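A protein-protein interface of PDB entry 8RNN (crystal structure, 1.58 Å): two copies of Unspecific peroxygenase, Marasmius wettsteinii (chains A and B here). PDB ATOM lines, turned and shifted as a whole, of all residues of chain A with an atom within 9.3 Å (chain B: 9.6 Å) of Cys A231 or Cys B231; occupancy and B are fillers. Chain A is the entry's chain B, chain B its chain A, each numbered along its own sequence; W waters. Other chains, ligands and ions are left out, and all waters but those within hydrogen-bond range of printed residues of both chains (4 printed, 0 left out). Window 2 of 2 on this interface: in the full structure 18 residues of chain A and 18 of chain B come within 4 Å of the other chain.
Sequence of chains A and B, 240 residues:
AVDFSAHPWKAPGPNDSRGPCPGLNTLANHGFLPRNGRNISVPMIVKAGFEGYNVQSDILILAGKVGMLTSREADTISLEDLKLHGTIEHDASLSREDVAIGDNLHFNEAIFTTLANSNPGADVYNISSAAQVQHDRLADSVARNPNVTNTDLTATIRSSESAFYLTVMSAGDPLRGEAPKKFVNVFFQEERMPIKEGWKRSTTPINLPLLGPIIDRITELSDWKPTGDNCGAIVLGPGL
The side-chain sulfur (SG) of Cys B231 is disulfide-bonded to the side-chain sulfur (SG) of Cys A231 (2.1 Å). SG of Cys B231 lies within hydrogen-bond range of N of Gly A232 (3.7 Å).
OD2 of Asp B229 lies close to N of Cys B231.
Among the printed residues, pairs that only touch across the chains: Gly A232 with Ala B233, Ala A233 with Gly B232 and Ala A233 with Ala B233.
Printed residues of chain B within 4 Å of Cys A231: Cys B231 (2.1 Å). Gly A232 touches just these residues of chain B: Cys B231 (3.7 Å) and Ala B233 (3.5 Å). Of chain B, only Gly B232 (3.4 Å) and Ala B233 (3.6 Å) come within 4 Å of Ala A233. Cys B231 touches just these residues of chain A: Cys A231 (2.1 Å) and Gly A232 (3.7 Å). Of the printed residues of chain A, Gly B232 touches Ala A233 (3.4 Å). Ala B233 touches two residues of chain A. The nearest residue of chain B that does not touch Cys A231 is Gly B232 (4.2 Å).
Of the 18 printed residues of chain B, 3 touch a printed residue of chain A. Hydrophobic or aromatic side chains of chain B that line the printed part of chain A: Ala B233. Of the 18 printed residues of chain A, 3 touch a printed residue of chain B. Hydrophobic or aromatic side chains of chain A within 4 Å of the printed part of chain B: Ala A233. Along chain A the printed residues that touch a printed residue of chain B span positions 231 to 233. Among the printed residues, 5 pairs touch across the chains. Among the printed residues, no Asp or Glu carboxylate lies within 4 Å of a Lys or Arg side-chain nitrogen of the other chain.
Cys B231 touches its own counterpart, Cys A231. Gly A232 touches Cys B231, but with the chains exchanged Cys A231 does not touch Gly B232 (4.2 Å). Gly A232 touches Ala B233, and with the chains exchanged Ala A233 touches Gly B232. Ala A233 touches its own counterpart, Ala B233. Positions printed for both chains: 86, 149, 150, 151, 152, 153, 154, 224, 226, 227, 228, 229, 230, 231, 232, 233, 234 and 235.
Water W2 lies within hydrogen-bond range of the backbone carbonyl oxygen of Gly B232 (2.6 Å), the backbone carbonyl oxygen of Ile A234 (2.9 Å) and the backbone NH of Ile B234 (3.2 Å). Water W4 lies within hydrogen-bond range of O of Gly A232 (2.8 Å), O of Ile B234 (3.0 Å) and N of Ile A234 (3.2 Å). Water W1 lies within hydrogen-bond range of N of Gly B232 (2.8 Å) and SG of Cys A231 (3.7 Å). Water W3 bridges the backbone NH of Gly A232 (2.9 Å) and the side-chain sulfur of Cys B231 (3.8 Å).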
ATOM      1  N   GLY A  86       3.708  10.491 -20.154  1.00  0.00           N
ATOM      2  CA  GLY A  86       2.796   9.394 -19.884  1.00  0.00           C
ATOM      3  C   GLY A  86       2.171   9.439 -18.492  1.00  0.00           C
ATOM      4  O   GLY A  86       1.422   8.525 -18.172  1.00  0.00           O
ATOM      5  N   THR A 149       1.260   8.043 -28.745  1.00  0.00           N
ATOM      6  CA  THR A 149       0.291   7.461 -27.833  1.00  0.00           C
ATOM      7  C   THR A 149      -0.958   8.343 -27.849  1.00  0.00           C
ATOM      8  O   THR A 149      -0.868   9.551 -27.633  1.00  0.00           O
ATOM      9  CB  THR A 149       0.868   7.324 -26.421  1.00  0.00           C
ATOM     10  OG1 THR A 149       2.046   6.507 -26.419  1.00  0.00           O
ATOM     11  CG2 THR A 149      -0.136   6.754 -25.441  1.00  0.00           C
ATOM     12  N   ASN A 150      -2.102   7.726 -28.160  1.00  0.00           N
ATOM     13  CA  ASN A 150      -3.364   8.417 -28.372  1.00  0.00           C
ATOM     14  C   ASN A 150      -4.497   7.515 -27.878  1.00  0.00           C
ATOM     15  O   ASN A 150      -4.865   6.545 -28.533  1.00  0.00           O
ATOM     16  CB  ASN A 150      -3.541   8.846 -29.831  1.00  0.00           C
ATOM     17  CG  ASN A 150      -4.954   9.256 -30.163  1.00  0.00           C
ATOM     18  OD1 ASN A 150      -5.530  10.120 -29.511  1.00  0.00           O
ATOM     19  ND2 ASN A 150      -5.515   8.659 -31.203  1.00  0.00           N
ATOM     20  N   THR A 151      -4.981   7.810 -26.668  1.00  0.00           N
ATOM     21  CA  THR A 151      -5.923   6.971 -25.943  1.00  0.00           C
ATOM     22  C   THR A 151      -7.129   7.805 -25.510  1.00  0.00           C
ATOM     23  O   THR A 151      -7.116   9.032 -25.623  1.00  0.00           O
ATOM     24  CB  THR A 151      -5.257   6.356 -24.704  1.00  0.00           C
ATOM     25  OG1 THR A 151      -4.969   7.411 -23.778  1.00  0.00           O
ATOM     26  CG2 THR A 151      -3.991   5.588 -25.023  1.00  0.00           C
ATOM     27  N   ASP A 152      -8.170   7.146 -24.981  1.00  0.00           N
ATOM     28  CA  ASP A 152      -9.317   7.856 -24.424  1.00  0.00           C
ATOM     29  C   ASP A 152      -8.859   8.890 -23.394  1.00  0.00           C
ATOM     30  O   ASP A 152      -9.362  10.018 -23.348  1.00  0.00           O
ATOM     31  CB  ASP A 152     -10.310   6.905 -23.747  1.00  0.00           C
ATOM     32  CG  ASP A 152     -11.047   5.934 -24.658  1.00  0.00           C
ATOM     33  OD1 ASP A 152     -11.187   6.228 -25.853  1.00  0.00           O
ATOM     34  OD2 ASP A 152     -11.484   4.883 -24.148  1.00  0.00           O
ATOM     35  N   LEU A 153      -7.885   8.482 -22.571  1.00  0.00           N
ATOM     36  CA  LEU A 153      -7.382   9.357 -21.524  1.00  0.00           C
ATOM     37  C   LEU A 153      -6.638  10.556 -22.114  1.00  0.00           C
ATOM     38  O   LEU A 153      -6.913  11.683 -21.702  1.00  0.00           O
ATOM     39  CB  LEU A 153      -6.489   8.577 -20.559  1.00  0.00           C
ATOM     40  CG  LEU A 153      -5.905   9.394 -19.407  1.00  0.00           C
ATOM     41  CD1 LEU A 153      -6.987  10.100 -18.590  1.00  0.00           C
ATOM     42  CD2 LEU A 153      -5.072   8.493 -18.513  1.00  0.00           C
ATOM     43  N   THR A 154      -5.697  10.336 -23.043  1.00  0.00           N
ATOM     44  CA  THR A 154      -4.952  11.472 -23.587  1.00  0.00           C
ATOM     45  C   THR A 154      -5.890  12.426 -24.324  1.00  0.00           C
ATOM     46  O   THR A 154      -5.709  13.637 -24.255  1.00  0.00           O
ATOM     47  CB  THR A 154      -3.772  11.071 -24.478  1.00  0.00           C
ATOM     48  OG1 THR A 154      -4.231  10.401 -25.654  1.00  0.00           O
ATOM     49  CG2 THR A 154      -2.770  10.230 -23.723  1.00  0.00           C
ATOM     50  N   TRP A 224     -12.357  12.297 -33.630  1.00  0.00           N
ATOM     51  CA  TRP A 224     -11.295  11.547 -32.976  1.00  0.00           C
ATOM     52  C   TRP A 224     -11.535  10.037 -33.067  1.00  0.00           C
ATOM     53  O   TRP A 224     -12.668   9.588 -33.007  1.00  0.00           O
ATOM     54  CB  TRP A 224     -11.200  12.017 -31.522  1.00  0.00           C
ATOM     55  CG  TRP A 224     -10.167  11.294 -30.723  1.00  0.00           C
ATOM     56  CD1 TRP A 224      -8.830  11.564 -30.648  1.00  0.00           C
ATOM     57  CD2 TRP A 224     -10.382  10.107 -29.949  1.00  0.00           C
ATOM     58  NE1 TRP A 224      -8.207  10.645 -29.852  1.00  0.00           N
ATOM     59  CE2 TRP A 224      -9.134   9.739 -29.404  1.00  0.00           C
ATOM     60  CE3 TRP A 224     -11.504   9.320 -29.668  1.00  0.00           C
ATOM     61  CZ2 TRP A 224      -8.982   8.626 -28.582  1.00  0.00           C
ATOM     62  CZ3 TRP A 224     -11.361   8.243 -28.824  1.00  0.00           C
ATOM     63  CH2 TRP A 224     -10.118   7.901 -28.292  1.00  0.00           C
ATOM     64  N   PRO A 226      -9.236   6.361 -31.376  1.00  0.00           N
ATOM     65  CA  PRO A 226      -8.052   5.891 -30.652  1.00  0.00           C
ATOM     66  C   PRO A 226      -6.983   5.319 -31.576  1.00  0.00           C
ATOM     67  O   PRO A 226      -7.286   4.929 -32.704  1.00  0.00           O
ATOM     68  CB  PRO A 226      -8.594   4.775 -29.741  1.00  0.00           C
ATOM     69  CG  PRO A 226      -9.874   4.318 -30.406  1.00  0.00           C
ATOM     70  CD  PRO A 226     -10.435   5.566 -31.058  1.00  0.00           C
ATOM     71  N   THR A 227      -5.751   5.240 -31.053  1.00  0.00           N
ATOM     72  CA  THR A 227      -4.625   4.569 -31.691  1.00  0.00           C
ATOM     73  C   THR A 227      -4.204   3.323 -30.902  1.00  0.00           C
ATOM     74  O   THR A 227      -4.072   3.386 -29.687  1.00  0.00           O
ATOM     75  CB  THR A 227      -3.424   5.521 -31.763  1.00  0.00           C
ATOM     76  OG1 THR A 227      -3.774   6.673 -32.532  1.00  0.00           O
ATOM     77  CG2 THR A 227      -2.186   4.887 -32.358  1.00  0.00           C
ATOM     78  N   GLY A 228      -3.991   2.192 -31.597  1.00  0.00           N
ATOM     79  CA  GLY A 228      -3.344   1.018 -31.022  1.00  0.00           C
ATOM     80  C   GLY A 228      -4.146   0.373 -29.890  1.00  0.00           C
ATOM     81  O   GLY A 228      -5.354   0.217 -30.004  1.00  0.00           O
ATOM     82  N   ASP A 229      -3.443   0.013 -28.808  1.00  0.00           N
ATOM     83  CA  ASP A 229      -4.013  -0.661 -27.648  1.00  0.00           C
ATOM     84  C   ASP A 229      -5.130   0.137 -26.974  1.00  0.00           C
ATOM     85  O   ASP A 229      -5.956  -0.457 -26.282  1.00  0.00           O
ATOM     86  CB  ASP A 229      -2.945  -0.919 -26.579  1.00  0.00           C
ATOM     87  CG  ASP A 229      -1.995  -2.066 -26.878  1.00  0.00           C
ATOM     88  OD1 ASP A 229      -2.024  -2.585 -28.014  1.00  0.00           O
ATOM     89  OD2 ASP A 229      -1.237  -2.439 -25.965  1.00  0.00           O
ATOM     90  N   ASN A 230      -5.107   1.474 -27.081  1.00  0.00           N
ATOM     91  CA  ASN A 230      -6.006   2.353 -26.341  1.00  0.00           C
ATOM     92  C   ASN A 230      -5.948   2.030 -24.844  1.00  0.00           C
ATOM     93  O   ASN A 230      -6.979   1.891 -24.186  1.00  0.00           O
ATOM     94  CB  ASN A 230      -7.429   2.264 -26.892  1.00  0.00           C
ATOM     95  CG  ASN A 230      -8.358   3.358 -26.400  1.00  0.00           C
ATOM     96  OD1 ASN A 230      -7.930   4.368 -25.833  1.00  0.00           O
ATOM     97  ND2 ASN A 230      -9.648   3.165 -26.622  1.00  0.00           N
ATOM     98  N   CYS A 231      -4.729   1.910 -24.315  1.00  0.00           N
ATOM     99  CA  CYS A 231      -4.526   1.612 -22.901  1.00  0.00           C
ATOM    100  C   CYS A 231      -4.330   2.919 -22.131  1.00  0.00           C
ATOM    101  O   CYS A 231      -3.316   3.584 -22.314  1.00  0.00           O
ATOM    102  CB  CYS A 231      -3.337   0.675 -22.733  1.00  0.00           C
ATOM    103  SG  CYS A 231      -2.932   0.261 -21.012  1.00  0.00           S
ATOM    104  N   GLY A 232      -5.287   3.254 -21.256  1.00  0.00           N
ATOM    105  CA  GLY A 232      -5.264   4.503 -20.506  1.00  0.00           C
ATOM    106  C   GLY A 232      -4.477   4.409 -19.199  1.00  0.00           C
ATOM    107  O   GLY A 232      -4.907   4.973 -18.195  1.00  0.00           O
ATOM    108  N   ALA A 233      -3.325   3.717 -19.227  1.00  0.00           N
ATOM    109  CA  ALA A 233      -2.472   3.518 -18.060  1.00  0.00           C
ATOM    110  C   ALA A 233      -1.488   4.674 -17.922  1.00  0.00           C
ATOM    111  O   ALA A 233      -0.729   4.934 -18.847  1.00  0.00           O
ATOM    112  CB  ALA A 233      -1.714   2.224 -18.176  1.00  0.00           C
ATOM    113  N   ILE A 234      -1.506   5.359 -16.771  1.00  0.00           N
ATOM    114  CA  ILE A 234      -0.546   6.416 -16.497  1.00  0.00           C
ATOM    115  C   ILE A 234       0.726   5.830 -15.883  1.00  0.00           C
ATOM    116  O   ILE A 234       0.713   4.785 -15.229  1.00  0.00           O
ATOM    117  CB  ILE A 234      -1.142   7.521 -15.603  1.00  0.00           C
ATOM    118  CG1 ILE A 234      -1.495   7.031 -14.197  1.00  0.00           C
ATOM    119  CG2 ILE A 234      -2.324   8.193 -16.274  1.00  0.00           C
ATOM    120  CD1 ILE A 234      -1.559   8.143 -13.178  1.00  0.00           C
ATOM    121  N   VAL A 235       1.830   6.562 -16.090  1.00  0.00           N
ATOM    122  CA  VAL A 235       3.103   6.334 -15.426  1.00  0.00           C
ATOM    123  C   VAL A 235       2.990   6.806 -13.973  1.00  0.00           C
ATOM    124  O   VAL A 235       2.559   7.928 -13.715  1.00  0.00           O
ATOM    125  CB  VAL A 235       4.215   7.073 -16.196  1.00  0.00           C
ATOM    126  CG1 VAL A 235       5.533   7.104 -15.444  1.00  0.00           C
ATOM    127  CG2 VAL A 235       4.397   6.491 -17.590  1.00  0.00           C
ATOM    128  N   GLY B  86      -9.269  -0.671  -7.863  1.00  0.00           N
ATOM    129  CA  GLY B  86      -8.610  -0.366  -9.120  1.00  0.00           C
ATOM    130  C   GLY B  86      -7.653   0.820  -9.071  1.00  0.00           C
ATOM    131  O   GLY B  86      -7.098   1.168 -10.110  1.00  0.00           O
ATOM    132  N   THR B 149      -9.948  -8.990 -12.227  1.00  0.00           N
ATOM    133  CA  THR B 149      -8.936  -8.219 -12.932  1.00  0.00           C
ATOM    134  C   THR B 149      -7.571  -8.757 -12.519  1.00  0.00           C
ATOM    135  O   THR B 149      -7.278  -8.824 -11.329  1.00  0.00           O
ATOM    136  CB  THR B 149      -9.068  -6.711 -12.656  1.00  0.00           C
ATOM    137  OG1 THR B 149     -10.346  -6.230 -13.068  1.00  0.00           O
ATOM    138  CG2 THR B 149      -8.008  -5.898 -13.357  1.00  0.00           C
ATOM    139  N   ASN B 150      -6.750  -9.118 -13.513  1.00  0.00           N
ATOM    140  CA  ASN B 150      -5.430  -9.692 -13.309  1.00  0.00           C
ATOM    141  C   ASN B 150      -4.494  -9.145 -14.386  1.00  0.00           C
ATOM    142  O   ASN B 150      -4.571  -9.552 -15.545  1.00  0.00           O
ATOM    143  CB  ASN B 150      -5.489 -11.222 -13.363  1.00  0.00           C
ATOM    144  CG  ASN B 150      -4.117 -11.855 -13.407  1.00  0.00           C
ATOM    145  OD1 ASN B 150      -3.263 -11.554 -12.570  1.00  0.00           O
ATOM    146  ND2 ASN B 150      -3.853 -12.693 -14.403  1.00  0.00           N
ATOM    147  N   THR B 151      -3.666  -8.168 -14.021  1.00  0.00           N
ATOM    148  CA  THR B 151      -2.756  -7.509 -14.953  1.00  0.00           C
ATOM    149  C   THR B 151      -1.320  -7.606 -14.429  1.00  0.00           C
ATOM    150  O   THR B 151      -1.110  -8.005 -13.288  1.00  0.00           O
ATOM    151  CB  THR B 151      -3.140  -6.032 -15.127  1.00  0.00           C
ATOM    152  OG1 THR B 151      -2.916  -5.356 -13.889  1.00  0.00           O
ATOM    153  CG2 THR B 151      -4.581  -5.810 -15.528  1.00  0.00           C
ATOM    154  N   ASP B 152      -0.323  -7.239 -15.251  1.00  0.00           N
ATOM    155  CA  ASP B 152       1.065  -7.166 -14.818  1.00  0.00           C
ATOM    156  C   ASP B 152       1.163  -6.305 -13.563  1.00  0.00           C
ATOM    157  O   ASP B 152       1.921  -6.606 -12.649  1.00  0.00           O
ATOM    158  CB  ASP B 152       1.967  -6.513 -15.878  1.00  0.00           C
ATOM    159  CG  ASP B 152       2.273  -7.360 -17.096  1.00  0.00           C
ATOM    160  OD1 ASP B 152       2.169  -8.582 -16.991  1.00  0.00           O
ATOM    161  OD2 ASP B 152       2.610  -6.777 -18.137  1.00  0.00           O
ATOM    162  N   LEU B 153       0.411  -5.195 -13.564  1.00  0.00           N
ATOM    163  CA  LEU B 153       0.451  -4.252 -12.458  1.00  0.00           C
ATOM    164  C   LEU B 153      -0.129  -4.899 -11.198  1.00  0.00           C
ATOM    165  O   LEU B 153       0.504  -4.820 -10.148  1.00  0.00           O
ATOM    166  CB  LEU B 153      -0.269  -2.945 -12.803  1.00  0.00           C
ATOM    167  CG  LEU B 153      -0.334  -1.925 -11.661  1.00  0.00           C
ATOM    168  CD1 LEU B 153       1.060  -1.516 -11.205  1.00  0.00           C
ATOM    169  CD2 LEU B 153      -1.134  -0.702 -12.048  1.00  0.00           C
ATOM    170  N   THR B 154      -1.328  -5.504 -11.264  1.00  0.00           N
ATOM    171  CA  THR B 154      -1.884  -6.099 -10.050  1.00  0.00           C
ATOM    172  C   THR B 154      -0.972  -7.216  -9.544  1.00  0.00           C
ATOM    173  O   THR B 154      -0.820  -7.399  -8.339  1.00  0.00           O
ATOM    174  CB  THR B 154      -3.326  -6.604 -10.212  1.00  0.00           C
ATOM    175  OG1 THR B 154      -3.396  -7.674 -11.168  1.00  0.00           O
ATOM    176  CG2 THR B 154      -4.273  -5.489 -10.588  1.00  0.00           C
ATOM    177  N   TRP B 224       2.918 -17.176 -12.905  1.00  0.00           N
ATOM    178  CA  TRP B 224       1.934 -16.180 -13.309  1.00  0.00           C
ATOM    179  C   TRP B 224       1.927 -16.053 -14.827  1.00  0.00           C
ATOM    180  O   TRP B 224       2.983 -16.063 -15.458  1.00  0.00           O
ATOM    181  CB  TRP B 224       2.216 -14.810 -12.678  1.00  0.00           C
ATOM    182  CG  TRP B 224       1.179 -13.785 -13.030  1.00  0.00           C
ATOM    183  CD1 TRP B 224       0.010 -13.554 -12.364  1.00  0.00           C
ATOM    184  CD2 TRP B 224       1.162 -12.902 -14.168  1.00  0.00           C
ATOM    185  NE1 TRP B 224      -0.693 -12.552 -12.966  1.00  0.00           N
ATOM    186  CE2 TRP B 224      -0.039 -12.168 -14.105  1.00  0.00           C
ATOM    187  CE3 TRP B 224       2.037 -12.665 -15.234  1.00  0.00           C
ATOM    188  CZ2 TRP B 224      -0.367 -11.185 -15.041  1.00  0.00           C
ATOM    189  CZ3 TRP B 224       1.694 -11.715 -16.176  1.00  0.00           C
ATOM    190  CH2 TRP B 224       0.500 -11.002 -16.092  1.00  0.00           C
ATOM    191  N   PRO B 226      -0.504 -13.804 -18.087  1.00  0.00           N
ATOM    192  CA  PRO B 226      -1.633 -12.944 -18.444  1.00  0.00           C
ATOM    193  C   PRO B 226      -2.849 -13.788 -18.821  1.00  0.00           C
ATOM    194  O   PRO B 226      -2.699 -14.896 -19.341  1.00  0.00           O
ATOM    195  CB  PRO B 226      -1.138 -12.103 -19.628  1.00  0.00           C
ATOM    196  CG  PRO B 226       0.032 -12.888 -20.179  1.00  0.00           C
ATOM    197  CD  PRO B 226       0.634 -13.642 -19.011  1.00  0.00           C
ATOM    198  N   THR B 227      -4.038 -13.275 -18.498  1.00  0.00           N
ATOM    199  CA  THR B 227      -5.282 -14.026 -18.601  1.00  0.00           C
ATOM    200  C   THR B 227      -6.299 -13.270 -19.453  1.00  0.00           C
ATOM    201  O   THR B 227      -7.324 -13.831 -19.835  1.00  0.00           O
ATOM    202  CB  THR B 227      -5.864 -14.328 -17.211  1.00  0.00           C
ATOM    203  OG1 THR B 227      -5.884 -13.137 -16.424  1.00  0.00           O
ATOM    204  CG2 THR B 227      -5.077 -15.392 -16.467  1.00  0.00           C
ATOM    205  N   GLY B 228      -6.055 -11.977 -19.677  1.00  0.00           N
ATOM    206  CA  GLY B 228      -6.979 -11.096 -20.377  1.00  0.00           C
ATOM    207  C   GLY B 228      -6.370  -9.710 -20.606  1.00  0.00           C
ATOM    208  O   GLY B 228      -5.218  -9.606 -21.025  1.00  0.00           O
ATOM    209  N   ASP B 229      -7.124  -8.663 -20.243  1.00  0.00           N
ATOM    210  CA  ASP B 229      -6.907  -7.287 -20.693  1.00  0.00           C
ATOM    211  C   ASP B 229      -5.428  -6.865 -20.650  1.00  0.00           C
ATOM    212  O   ASP B 229      -4.850  -6.496 -21.675  1.00  0.00           O
ATOM    213  CB  ASP B 229      -7.820  -6.353 -19.887  1.00  0.00           C
ATOM    214  CG  ASP B 229      -7.625  -4.879 -20.199  1.00  0.00           C
ATOM    215  OD1 ASP B 229      -7.834  -4.496 -21.367  1.00  0.00           O
ATOM    216  OD2 ASP B 229      -7.263  -4.131 -19.272  1.00  0.00           O
ATOM    217  N   ASN B 230      -4.844  -6.895 -19.452  1.00  0.00           N
ATOM    218  CA  ASN B 230      -3.435  -6.621 -19.167  1.00  0.00           C
ATOM    219  C   ASN B 230      -3.048  -5.138 -19.220  1.00  0.00           C
ATOM    220  O   ASN B 230      -1.885  -4.818 -18.989  1.00  0.00           O
ATOM    221  CB  ASN B 230      -2.425  -7.432 -19.997  1.00  0.00           C
ATOM    222  CG  ASN B 230      -1.204  -7.772 -19.164  1.00  0.00           C
ATOM    223  OD1 ASN B 230      -1.248  -7.604 -17.953  1.00  0.00           O
ATOM    224  ND2 ASN B 230      -0.132  -8.267 -19.764  1.00  0.00           N
ATOM    225  N   CYS B 231      -4.006  -4.224 -19.423  1.00  0.00           N
ATOM    226  CA  CYS B 231      -3.753  -2.790 -19.340  1.00  0.00           C
ATOM    227  C   CYS B 231      -3.675  -2.371 -17.872  1.00  0.00           C
ATOM    228  O   CYS B 231      -4.671  -2.455 -17.154  1.00  0.00           O
ATOM    229  CB  CYS B 231      -4.855  -2.023 -20.068  1.00  0.00           C
ATOM    230  SG  CYS B 231      -4.688  -0.213 -20.028  1.00  0.00           S
ATOM    231  N   GLY B 232      -2.500  -1.890 -17.446  1.00  0.00           N
ATOM    232  CA  GLY B 232      -2.261  -1.510 -16.062  1.00  0.00           C
ATOM    233  C   GLY B 232      -2.735  -0.088 -15.754  1.00  0.00           C
ATOM    234  O   GLY B 232      -1.981   0.684 -15.166  1.00  0.00           O
ATOM    235  N   ALA B 233      -3.993   0.217 -16.123  1.00  0.00           N
ATOM    236  CA  ALA B 233      -4.601   1.528 -15.931  1.00  0.00           C
ATOM    237  C   ALA B 233      -5.215   1.628 -14.540  1.00  0.00           C
ATOM    238  O   ALA B 233      -6.101   0.849 -14.223  1.00  0.00           O
ATOM    239  CB  ALA B 233      -5.666   1.758 -16.971  1.00  0.00           C
ATOM    240  N   ILE B 234      -4.737   2.586 -13.731  1.00  0.00           N
ATOM    241  CA  ILE B 234      -5.291   2.802 -12.406  1.00  0.00           C
ATOM    242  C   ILE B 234      -6.452   3.792 -12.490  1.00  0.00           C
ATOM    243  O   ILE B 234      -6.503   4.660 -13.377  1.00  0.00           O
ATOM    244  CB  ILE B 234      -4.221   3.268 -11.396  1.00  0.00           C
ATOM    245  CG1 ILE B 234      -3.627   4.635 -11.749  1.00  0.00           C
ATOM    246  CG2 ILE B 234      -3.133   2.215 -11.216  1.00  0.00           C
ATOM    247  CD1 ILE B 234      -3.021   5.346 -10.551  1.00  0.00           C
ATOM    248  N   VAL B 235      -7.364   3.676 -11.516  1.00  0.00           N
ATOM    249  CA  VAL B 235      -8.417   4.639 -11.254  1.00  0.00           C
ATOM    250  C   VAL B 235      -7.795   5.885 -10.623  1.00  0.00           C
ATOM    251  O   VAL B 235      -7.067   5.769  -9.637  1.00  0.00           O
ATOM    252  CB  VAL B 235      -9.498   4.004 -10.350  1.00  0.00           C
ATOM    253  CG1 VAL B 235     -10.505   5.011  -9.835  1.00  0.00           C
ATOM    254  CG2 VAL B 235     -10.214   2.846 -11.035  1.00  0.00           C
HETATM  255  O   HOH W   1      -0.325  -1.638 -19.266  1.00  0.00           O
HETATM  256  O   HOH W   2      -1.647   3.188 -14.482  1.00  0.00           O
HETATM  257  O   HOH W   3      -7.796   1.837 -20.759  1.00  0.00           O
HETATM  258  O   HOH W   4      -4.419   5.186 -15.448  1.00  0.00           O
